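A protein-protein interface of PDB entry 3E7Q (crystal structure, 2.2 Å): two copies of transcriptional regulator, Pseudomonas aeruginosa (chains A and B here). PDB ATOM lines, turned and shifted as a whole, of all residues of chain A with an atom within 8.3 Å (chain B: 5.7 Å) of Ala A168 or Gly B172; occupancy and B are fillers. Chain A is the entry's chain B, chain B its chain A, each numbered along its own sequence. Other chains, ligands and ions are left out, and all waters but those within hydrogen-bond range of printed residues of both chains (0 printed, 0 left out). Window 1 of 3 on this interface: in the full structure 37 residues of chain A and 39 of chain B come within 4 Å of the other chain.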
ATOM      1  N   TYR A 134     -29.700  25.799  -9.643  1.00  0.00           N
ATOM      2  CA  TYR A 134     -28.298  26.173  -9.671  1.00  0.00           C
ATOM      3  C   TYR A 134     -28.122  27.533 -10.431  1.00  0.00           C
ATOM      4  O   TYR A 134     -27.359  28.386 -10.020  1.00  0.00           O
ATOM      5  CB  TYR A 134     -27.467  25.010 -10.278  1.00  0.00           C
ATOM      6  CG  TYR A 134     -25.942  25.236 -10.395  1.00  0.00           C
ATOM      7  CD1 TYR A 134     -25.135  25.468  -9.275  1.00  0.00           C
ATOM      8  CD2 TYR A 134     -25.325  25.203 -11.658  1.00  0.00           C
ATOM      9  CE1 TYR A 134     -23.753  25.692  -9.416  1.00  0.00           C
ATOM     10  CE2 TYR A 134     -23.990  25.414 -11.817  1.00  0.00           C
ATOM     11  CZ  TYR A 134     -23.192  25.656 -10.700  1.00  0.00           C
ATOM     12  OH  TYR A 134     -21.837  25.828 -10.936  1.00  0.00           O
ATOM     13  N   TYR A 137     -29.151  30.263  -7.922  1.00  0.00           N
ATOM     14  CA  TYR A 137     -28.163  30.351  -6.875  1.00  0.00           C
ATOM     15  C   TYR A 137     -26.946  31.191  -7.350  1.00  0.00           C
ATOM     16  O   TYR A 137     -26.512  32.195  -6.701  1.00  0.00           O
ATOM     17  CB  TYR A 137     -27.784  28.923  -6.451  1.00  0.00           C
ATOM     18  CG  TYR A 137     -26.780  28.825  -5.322  1.00  0.00           C
ATOM     19  CD1 TYR A 137     -27.187  28.846  -3.994  1.00  0.00           C
ATOM     20  CD2 TYR A 137     -25.436  28.707  -5.589  1.00  0.00           C
ATOM     21  CE1 TYR A 137     -26.284  28.742  -2.980  1.00  0.00           C
ATOM     22  CE2 TYR A 137     -24.492  28.662  -4.574  1.00  0.00           C
ATOM     23  CZ  TYR A 137     -24.920  28.679  -3.271  1.00  0.00           C
ATOM     24  OH  TYR A 137     -23.992  28.556  -2.287  1.00  0.00           O
ATOM     25  N   ARG A 138     -26.425  30.810  -8.500  1.00  0.00           N
ATOM     26  CA  ARG A 138     -25.335  31.583  -9.154  1.00  0.00           C
ATOM     27  C   ARG A 138     -25.719  33.032  -9.530  1.00  0.00           C
ATOM     28  O   ARG A 138     -24.878  33.903  -9.426  1.00  0.00           O
ATOM     29  CB  ARG A 138     -24.779  30.842 -10.390  1.00  0.00           C
ATOM     30  CG  ARG A 138     -23.899  29.649 -10.044  1.00  0.00           C
ATOM     31  CD  ARG A 138     -23.323  28.993 -11.263  1.00  0.00           C
ATOM     32  NE  ARG A 138     -24.399  28.396 -12.080  1.00  0.00           N
ATOM     33  CZ  ARG A 138     -24.611  28.627 -13.370  1.00  0.00           C
ATOM     34  NH1 ARG A 138     -23.820  29.401 -14.080  1.00  0.00           N
ATOM     35  NH2 ARG A 138     -25.624  28.060 -13.966  1.00  0.00           N
ATOM     36  N   LEU A 141     -25.275  35.234  -6.611  1.00  0.00           N
ATOM     37  CA  LEU A 141     -23.868  35.485  -6.353  1.00  0.00           C
ATOM     38  C   LEU A 141     -23.247  36.350  -7.451  1.00  0.00           C
ATOM     39  O   LEU A 141     -22.384  37.152  -7.143  1.00  0.00           O
ATOM     40  CB  LEU A 141     -23.074  34.185  -6.138  1.00  0.00           C
ATOM     41  CG  LEU A 141     -23.287  33.445  -4.823  1.00  0.00           C
ATOM     42  CD1 LEU A 141     -22.739  32.043  -4.924  1.00  0.00           C
ATOM     43  CD2 LEU A 141     -22.640  34.243  -3.645  1.00  0.00           C
ATOM     44  N   LEU A 161     -18.055  33.483 -14.169  1.00  0.00           N
ATOM     45  CA  LEU A 161     -17.074  32.500 -13.851  1.00  0.00           C
ATOM     46  C   LEU A 161     -16.667  32.534 -12.413  1.00  0.00           C
ATOM     47  O   LEU A 161     -16.566  31.461 -11.802  1.00  0.00           O
ATOM     48  CB  LEU A 161     -15.876  32.593 -14.787  1.00  0.00           C
ATOM     49  CG  LEU A 161     -14.965  31.363 -14.861  1.00  0.00           C
ATOM     50  CD1 LEU A 161     -15.677  30.132 -15.514  1.00  0.00           C
ATOM     51  CD2 LEU A 161     -13.709  31.770 -15.542  1.00  0.00           C
ATOM     52  N   ALA A 162     -16.518  33.758 -11.861  1.00  0.00           N
ATOM     53  CA  ALA A 162     -16.298  33.979 -10.432  1.00  0.00           C
ATOM     54  C   ALA A 162     -17.403  33.342  -9.590  1.00  0.00           C
ATOM     55  O   ALA A 162     -17.145  32.730  -8.561  1.00  0.00           O
ATOM     56  CB  ALA A 162     -16.134  35.493 -10.141  1.00  0.00           C
ATOM     57  N   ALA A 163     -18.647  33.477 -10.025  1.00  0.00           N
ATOM     58  CA  ALA A 163     -19.773  32.911  -9.285  1.00  0.00           C
ATOM     59  C   ALA A 163     -19.758  31.349  -9.328  1.00  0.00           C
ATOM     60  O   ALA A 163     -20.081  30.707  -8.365  1.00  0.00           O
ATOM     61  CB  ALA A 163     -21.101  33.512  -9.768  1.00  0.00           C
ATOM     62  N   ILE A 164     -19.373  30.749 -10.437  1.00  0.00           N
ATOM     63  CA  ILE A 164     -19.184  29.337 -10.492  1.00  0.00           C
ATOM     64  C   ILE A 164     -18.098  28.893  -9.481  1.00  0.00           C
ATOM     65  O   ILE A 164     -18.267  27.880  -8.807  1.00  0.00           O
ATOM     66  CB  ILE A 164     -18.826  28.820 -11.939  1.00  0.00           C
ATOM     67  CG1 ILE A 164     -20.053  28.915 -12.844  1.00  0.00           C
ATOM     68  CG2 ILE A 164     -18.164  27.364 -11.890  1.00  0.00           C
ATOM     69  CD1 ILE A 164     -19.747  29.009 -14.346  1.00  0.00           C
ATOM     70  N   SER A 165     -17.039  29.666  -9.329  1.00  0.00           N
ATOM     71  CA  SER A 165     -15.948  29.317  -8.419  1.00  0.00           C
ATOM     72  C   SER A 165     -16.405  29.338  -6.967  1.00  0.00           C
ATOM     73  O   SER A 165     -16.142  28.421  -6.168  1.00  0.00           O
ATOM     74  CB  SER A 165     -14.793  30.307  -8.624  1.00  0.00           C
ATOM     75  OG  SER A 165     -13.685  30.018  -7.772  1.00  0.00           O
ATOM     76  N   LEU A 166     -17.018  30.448  -6.597  1.00  0.00           N
ATOM     77  CA  LEU A 166     -17.540  30.598  -5.281  1.00  0.00           C
ATOM     78  C   LEU A 166     -18.664  29.547  -4.917  1.00  0.00           C
ATOM     79  O   LEU A 166     -18.656  29.014  -3.803  1.00  0.00           O
ATOM     80  CB  LEU A 166     -18.020  32.053  -5.062  1.00  0.00           C
ATOM     81  CG  LEU A 166     -18.446  32.394  -3.619  1.00  0.00           C
ATOM     82  CD1 LEU A 166     -17.297  32.080  -2.573  1.00  0.00           C
ATOM     83  CD2 LEU A 166     -18.959  33.848  -3.527  1.00  0.00           C
ATOM     84  N   SER A 167     -19.619  29.300  -5.812  1.00  0.00           N
ATOM     85  CA  SER A 167     -20.600  28.222  -5.621  1.00  0.00           C
ATOM     86  C   SER A 167     -19.942  26.858  -5.442  1.00  0.00           C
ATOM     87  O   SER A 167     -20.330  26.099  -4.576  1.00  0.00           O
ATOM     88  CB  SER A 167     -21.578  28.118  -6.802  1.00  0.00           C
ATOM     89  OG  SER A 167     -22.188  29.378  -6.979  1.00  0.00           O
ATOM     90  N   ALA A 168     -18.964  26.563  -6.270  1.00  0.00           N
ATOM     91  CA  ALA A 168     -18.202  25.354  -6.140  1.00  0.00           C
ATOM     92  C   ALA A 168     -17.558  25.199  -4.750  1.00  0.00           C
ATOM     93  O   ALA A 168     -17.656  24.142  -4.136  1.00  0.00           O
ATOM     94  CB  ALA A 168     -17.183  25.242  -7.297  1.00  0.00           C
ATOM     95  N   LEU A 169     -16.950  26.264  -4.235  1.00  0.00           N
ATOM     96  CA  LEU A 169     -16.311  26.262  -2.919  1.00  0.00           C
ATOM     97  C   LEU A 169     -17.299  25.997  -1.795  1.00  0.00           C
ATOM     98  O   LEU A 169     -17.033  25.177  -0.921  1.00  0.00           O
ATOM     99  CB  LEU A 169     -15.586  27.559  -2.642  1.00  0.00           C
ATOM    100  CG  LEU A 169     -14.857  27.772  -1.279  1.00  0.00           C
ATOM    101  CD1 LEU A 169     -13.802  26.699  -1.082  1.00  0.00           C
ATOM    102  CD2 LEU A 169     -14.249  29.185  -1.179  1.00  0.00           C
ATOM    103  N   LEU A 170     -18.430  26.695  -1.835  1.00  0.00           N
ATOM    104  CA  LEU A 170     -19.553  26.524  -0.910  1.00  0.00           C
ATOM    105  C   LEU A 170     -20.121  25.145  -0.906  1.00  0.00           C
ATOM    106  O   LEU A 170     -20.253  24.549   0.153  1.00  0.00           O
ATOM    107  CB  LEU A 170     -20.680  27.550  -1.193  1.00  0.00           C
ATOM    108  CG  LEU A 170     -20.284  28.915  -0.656  1.00  0.00           C
ATOM    109  CD1 LEU A 170     -20.937  30.072  -1.448  1.00  0.00           C
ATOM    110  CD2 LEU A 170     -20.654  28.926   0.807  1.00  0.00           C
ATOM    111  N   ASP A 171     -20.400  24.619  -2.104  1.00  0.00           N
ATOM    112  CA  ASP A 171     -20.853  23.228  -2.300  1.00  0.00           C
ATOM    113  C   ASP A 171     -19.931  22.226  -1.695  1.00  0.00           C
ATOM    114  O   ASP A 171     -20.379  21.299  -0.987  1.00  0.00           O
ATOM    115  CB  ASP A 171     -20.952  22.863  -3.800  1.00  0.00           C
ATOM    116  CG  ASP A 171     -22.204  23.352  -4.451  1.00  0.00           C
ATOM    117  OD1 ASP A 171     -23.049  23.923  -3.757  1.00  0.00           O
ATOM    118  OD2 ASP A 171     -22.318  23.244  -5.704  1.00  0.00           O
ATOM    119  N   GLY A 172     -18.650  22.349  -2.067  1.00  0.00           N
ATOM    120  CA  GLY A 172     -17.571  21.483  -1.575  1.00  0.00           C
ATOM    121  C   GLY A 172     -17.495  21.499  -0.082  1.00  0.00           C
ATOM    122  O   GLY A 172     -17.389  20.469   0.540  1.00  0.00           O
ATOM    123  N   LEU A 173     -17.520  22.689   0.506  1.00  0.00           N
ATOM    124  CA  LEU A 173     -17.510  22.839   1.949  1.00  0.00           C
ATOM    125  C   LEU A 173     -18.758  22.299   2.651  1.00  0.00           C
ATOM    126  O   LEU A 173     -18.685  21.698   3.723  1.00  0.00           O
ATOM    127  CB  LEU A 173     -17.318  24.313   2.305  1.00  0.00           C
ATOM    128  CG  LEU A 173     -15.944  24.940   1.967  1.00  0.00           C
ATOM    129  CD1 LEU A 173     -16.149  26.317   2.313  1.00  0.00           C
ATOM    130  CD2 LEU A 173     -14.736  24.298   2.731  1.00  0.00           C
ATOM    131  N   TRP A 174     -19.913  22.520   2.048  1.00  0.00           N
ATOM    132  CA  TRP A 174     -21.152  22.003   2.592  1.00  0.00           C
ATOM    133  C   TRP A 174     -21.113  20.457   2.611  1.00  0.00           C
ATOM    134  O   TRP A 174     -21.466  19.845   3.588  1.00  0.00           O
ATOM    135  CB  TRP A 174     -22.344  22.549   1.797  1.00  0.00           C
ATOM    136  CG  TRP A 174     -23.630  22.054   2.303  1.00  0.00           C
ATOM    137  CD1 TRP A 174     -24.357  22.559   3.343  1.00  0.00           C
ATOM    138  CD2 TRP A 174     -24.340  20.902   1.840  1.00  0.00           C
ATOM    139  NE1 TRP A 174     -25.474  21.789   3.560  1.00  0.00           N
ATOM    140  CE2 TRP A 174     -25.491  20.775   2.632  1.00  0.00           C
ATOM    141  CE3 TRP A 174     -24.098  19.954   0.845  1.00  0.00           C
ATOM    142  CZ2 TRP A 174     -26.402  19.761   2.443  1.00  0.00           C
ATOM    143  CZ3 TRP A 174     -25.027  18.918   0.648  1.00  0.00           C
ATOM    144  CH2 TRP A 174     -26.145  18.823   1.443  1.00  0.00           C
ATOM    145  N   LEU A 175     -20.656  19.850   1.512  1.00  0.00           N
ATOM    146  CA  LEU A 175     -20.549  18.420   1.377  1.00  0.00           C
ATOM    147  C   LEU A 175     -19.559  17.827   2.407  1.00  0.00           C
ATOM    148  O   LEU A 175     -19.868  16.860   3.102  1.00  0.00           O
ATOM    149  CB  LEU A 175     -20.173  18.066  -0.084  1.00  0.00           C
ATOM    150  CG  LEU A 175     -19.912  16.587  -0.467  1.00  0.00           C
ATOM    151  CD1 LEU A 175     -21.207  15.720  -0.289  1.00  0.00           C
ATOM    152  CD2 LEU A 175     -19.352  16.504  -1.904  1.00  0.00           C
ATOM    153  N   TRP A 196     -11.357  33.581   0.267  1.00  0.00           N
ATOM    154  CA  TRP A 196     -11.527  33.560  -1.165  1.00  0.00           C
ATOM    155  C   TRP A 196     -11.812  34.956  -1.770  1.00  0.00           C
ATOM    156  O   TRP A 196     -11.273  35.338  -2.804  1.00  0.00           O
ATOM    157  CB  TRP A 196     -12.728  32.657  -1.485  1.00  0.00           C
ATOM    158  CG  TRP A 196     -12.985  32.493  -2.916  1.00  0.00           C
ATOM    159  CD1 TRP A 196     -12.466  31.529  -3.684  1.00  0.00           C
ATOM    160  CD2 TRP A 196     -13.850  33.287  -3.785  1.00  0.00           C
ATOM    161  NE1 TRP A 196     -12.936  31.647  -4.965  1.00  0.00           N
ATOM    162  CE2 TRP A 196     -13.763  32.723  -5.068  1.00  0.00           C
ATOM    163  CE3 TRP A 196     -14.658  34.402  -3.604  1.00  0.00           C
ATOM    164  CZ2 TRP A 196     -14.438  33.235  -6.179  1.00  0.00           C
ATOM    165  CZ3 TRP A 196     -15.342  34.915  -4.710  1.00  0.00           C
ATOM    166  CH2 TRP A 196     -15.238  34.311  -5.982  1.00  0.00           C
ATOM    167  N   SER B 167      -9.396  21.662  -1.827  1.00  0.00           N
ATOM    168  CA  SER B 167     -10.156  20.418  -2.011  1.00  0.00           C
ATOM    169  C   SER B 167     -11.662  20.643  -2.174  1.00  0.00           C
ATOM    170  O   SER B 167     -12.285  19.972  -2.985  1.00  0.00           O
ATOM    171  CB  SER B 167      -9.982  19.431  -0.835  1.00  0.00           C
ATOM    172  OG  SER B 167      -8.633  19.067  -0.714  1.00  0.00           O
ATOM    173  N   ALA B 168     -12.238  21.526  -1.347  1.00  0.00           N
ATOM    174  CA  ALA B 168     -13.681  21.863  -1.427  1.00  0.00           C
ATOM    175  C   ALA B 168     -14.033  22.488  -2.782  1.00  0.00           C
ATOM    176  O   ALA B 168     -15.039  22.132  -3.421  1.00  0.00           O
ATOM    177  CB  ALA B 168     -14.089  22.792  -0.273  1.00  0.00           C
ATOM    178  N   LEU B 169     -13.170  23.359  -3.260  1.00  0.00           N
ATOM    179  CA  LEU B 169     -13.371  23.965  -4.566  1.00  0.00           C
ATOM    180  C   LEU B 169     -13.367  22.915  -5.707  1.00  0.00           C
ATOM    181  O   LEU B 169     -14.256  22.920  -6.534  1.00  0.00           O
ATOM    182  CB  LEU B 169     -12.333  25.031  -4.830  1.00  0.00           C
ATOM    183  CG  LEU B 169     -12.328  25.713  -6.197  1.00  0.00           C
ATOM    184  CD1 LEU B 169     -13.670  26.484  -6.468  1.00  0.00           C
ATOM    185  CD2 LEU B 169     -11.052  26.621  -6.345  1.00  0.00           C
ATOM    186  N   LEU B 170     -12.323  22.111  -5.772  1.00  0.00           N
ATOM    187  CA  LEU B 170     -12.197  21.002  -6.713  1.00  0.00           C
ATOM    188  C   LEU B 170     -13.377  20.027  -6.631  1.00  0.00           C
ATOM    189  O   LEU B 170     -13.894  19.628  -7.642  1.00  0.00           O
ATOM    190  CB  LEU B 170     -10.905  20.230  -6.485  1.00  0.00           C
ATOM    191  CG  LEU B 170      -9.637  20.878  -7.049  1.00  0.00           C
ATOM    192  CD1 LEU B 170      -8.413  20.550  -6.166  1.00  0.00           C
ATOM    193  CD2 LEU B 170      -9.450  20.503  -8.487  1.00  0.00           C
ATOM    194  N   ASP B 171     -13.770  19.654  -5.425  1.00  0.00           N
ATOM    195  CA  ASP B 171     -14.952  18.796  -5.233  1.00  0.00           C
ATOM    196  C   ASP B 171     -16.200  19.393  -5.845  1.00  0.00           C
ATOM    197  O   ASP B 171     -16.927  18.705  -6.570  1.00  0.00           O
ATOM    198  CB  ASP B 171     -15.271  18.612  -3.759  1.00  0.00           C
ATOM    199  CG  ASP B 171     -14.601  17.393  -3.173  1.00  0.00           C
ATOM    200  OD1 ASP B 171     -13.632  16.886  -3.790  1.00  0.00           O
ATOM    201  OD2 ASP B 171     -15.032  16.980  -2.056  1.00  0.00           O
ATOM    202  N   GLY B 172     -16.424  20.666  -5.512  1.00  0.00           N
ATOM    203  CA  GLY B 172     -17.618  21.424  -5.949  1.00  0.00           C
ATOM    204  C   GLY B 172     -17.634  21.531  -7.453  1.00  0.00           C
ATOM    205  O   GLY B 172     -18.689  21.385  -8.082  1.00  0.00           O
ATOM    206  N   LEU B 173     -16.465  21.800  -8.033  1.00  0.00           N
ATOM    207  CA  LEU B 173     -16.341  21.901  -9.477  1.00  0.00           C
ATOM    208  C   LEU B 173     -16.534  20.538 -10.144  1.00  0.00           C
ATOM    209  O   LEU B 173     -17.174  20.448 -11.151  1.00  0.00           O
ATOM    210  CB  LEU B 173     -14.986  22.484  -9.864  1.00  0.00           C
ATOM    211  CG  LEU B 173     -14.720  23.963  -9.634  1.00  0.00           C
ATOM    212  CD1 LEU B 173     -13.214  24.282  -9.851  1.00  0.00           C
ATOM    213  CD2 LEU B 173     -15.686  24.897 -10.440  1.00  0.00           C
ATOM    214  N   TRP B 174     -15.992  19.487  -9.542  1.00  0.00           N
ATOM    215  CA  TRP B 174     -16.137  18.152 -10.070  1.00  0.00           C
ATOM    216  C   TRP B 174     -17.640  17.778 -10.057  1.00  0.00           C
ATOM    217  O   TRP B 174     -18.173  17.287 -11.043  1.00  0.00           O
ATOM    218  CB  TRP B 174     -15.252  17.139  -9.295  1.00  0.00           C
ATOM    219  CG  TRP B 174     -15.415  15.788  -9.811  1.00  0.00           C
ATOM    220  CD1 TRP B 174     -14.826  15.238 -10.954  1.00  0.00           C
ATOM    221  CD2 TRP B 174     -16.318  14.770  -9.303  1.00  0.00           C
ATOM    222  NE1 TRP B 174     -15.288  13.964 -11.142  1.00  0.00           N
ATOM    223  CE2 TRP B 174     -16.207  13.654 -10.164  1.00  0.00           C
ATOM    224  CE3 TRP B 174     -17.226  14.713  -8.224  1.00  0.00           C
ATOM    225  CZ2 TRP B 174     -16.964  12.474  -9.972  1.00  0.00           C
ATOM    226  CZ3 TRP B 174     -17.959  13.527  -8.020  1.00  0.00           C
ATOM    227  CH2 TRP B 174     -17.834  12.432  -8.900  1.00  0.00           C
ATOM    228  N   LEU B 175     -18.327  18.087  -8.974  1.00  0.00           N
ATOM    229  CA  LEU B 175     -19.718  17.719  -8.862  1.00  0.00           C
ATOM    230  C   LEU B 175     -20.618  18.467  -9.858  1.00  0.00           C
ATOM    231  O   LEU B 175     -21.456  17.866 -10.532  1.00  0.00           O
ATOM    232  CB  LEU B 175     -20.213  17.972  -7.415  1.00  0.00           C
ATOM    233  CG  LEU B 175     -21.651  17.639  -6.991  1.00  0.00           C
ATOM    234  CD1 LEU B 175     -21.874  16.160  -7.098  1.00  0.00           C
ATOM    235  CD2 LEU B 175     -22.015  18.152  -5.585  1.00  0.00           C
ATOM    236  N   GLU B 176     -20.438  19.789  -9.950  1.00  0.00           N
ATOM    237  CA  GLU B 176     -21.291  20.541 -10.813  1.00  0.00           C
ATOM    238  C   GLU B 176     -21.062  20.183 -12.252  1.00  0.00           C
ATOM    239  O   GLU B 176     -21.965  20.253 -13.076  1.00  0.00           O
ATOM    240  CB  GLU B 176     -21.070  22.026 -10.675  1.00  0.00           C
ATOM    241  CG  GLU B 176     -22.121  22.752 -11.603  1.00  0.00           C
ATOM    242  CD  GLU B 176     -23.571  22.161 -11.427  1.00  0.00           C
ATOM    243  OE1 GLU B 176     -23.973  21.888 -10.231  1.00  0.00           O
ATOM    244  OE2 GLU B 176     -24.250  21.971 -12.474  1.00  0.00           O
ATOM    245  N   SER B 177     -19.833  19.819 -12.545  1.00  0.00           N
ATOM    246  CA  SER B 177     -19.516  19.445 -13.826  1.00  0.00           C
ATOM    247  C   SER B 177     -20.235  18.172 -14.215  1.00  0.00           C
ATOM    248  O   SER B 177     -20.611  17.998 -15.371  1.00  0.00           O
ATOM    249  CB  SER B 177     -18.018  19.217 -13.951  1.00  0.00           C
ATOM    250  OG  SER B 177     -17.837  19.049 -15.295  1.00  0.00           O
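Of the 11 printed residues of chain B, 5 touch a printed residue of chain A. Of the 20 printed residues of chain A, 7 touch a printed residue of chain B. Among the printed residues, 11 pairs touch across the chains.
Tyr A134 touches Glu B176 (OH to CG, 3.2 Å). Ile A164 touches Leu B173 (CG2 to CD2, 3.8 Å). CD1 of Leu B169 touches O of Ser A165 (3.2 Å). Leu B169 touches Ala A168 (O to CB, 3.8 Å). Ala A168 touches Gly B172 (O to CA, 3.3 Å). Leu B173 touches Ala A168 (CD2 to CB, 3.5 Å). Ala B168 touches Leu A169 (CB to O, 3.8 Å). Leu A169 touches Leu B169 (N to CD1, 3.97 Å). Gly A172 touches Ala B168 (CA to O, 3.2 Å). Ala B168 touches Leu A173.
O of Ala A168 sits close to O of Ala B168, at 3.4 Å.
NE1 of Trp A196 is in hydrogen-bond range of OG of Ser A165, 3.3 Å away.
Ala A168 touches its own counterpart, Ala B168. Ala A168 touches Gly B172, and with the chains exchanged Gly A172 touches Ala B168. Ala A168 touches Leu B173, and with the chains exchanged Leu A173 touches Ala B168. Leu B169 touches its own counterpart, Leu A169. Positions printed for both chains: 167, 168, 169, 170, 171, 172, 173, 174 and 175. Of the 11 pairs that touch across the chains among the printed residues, 8 have their exchanged pair printed and touching as well.
Of chain B, only Ala B168, Leu B169, Gly B172 and Leu B173 come within 4 Å of Ala A168. Of the printed residues of chain B, Tyr A134 touches Glu B176. Printed residues of chain B within 4 Å of Leu A173: Ala B168 (3.4 Å). Of the printed residues of chain A, Leu B173 touches Ile A164 (3.8 Å) and Ala A168 (3.5 Å). Printed residues of chain B within 4 Å of Gly A172: Ala B168. Of the printed residues of chain B, Leu A169 touches Ala B168 and Leu B169. Leu B175 touches none of the printed residues of chain A. Trp A174 touches none of the printed residues of chain B. The nearest residue of chain A that does not touch Gly B172 is Gly A172 (4.1 Å). The nearest printed residue of chain A that does not touch Leu B173 is Ser A165 (4.9 Å).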
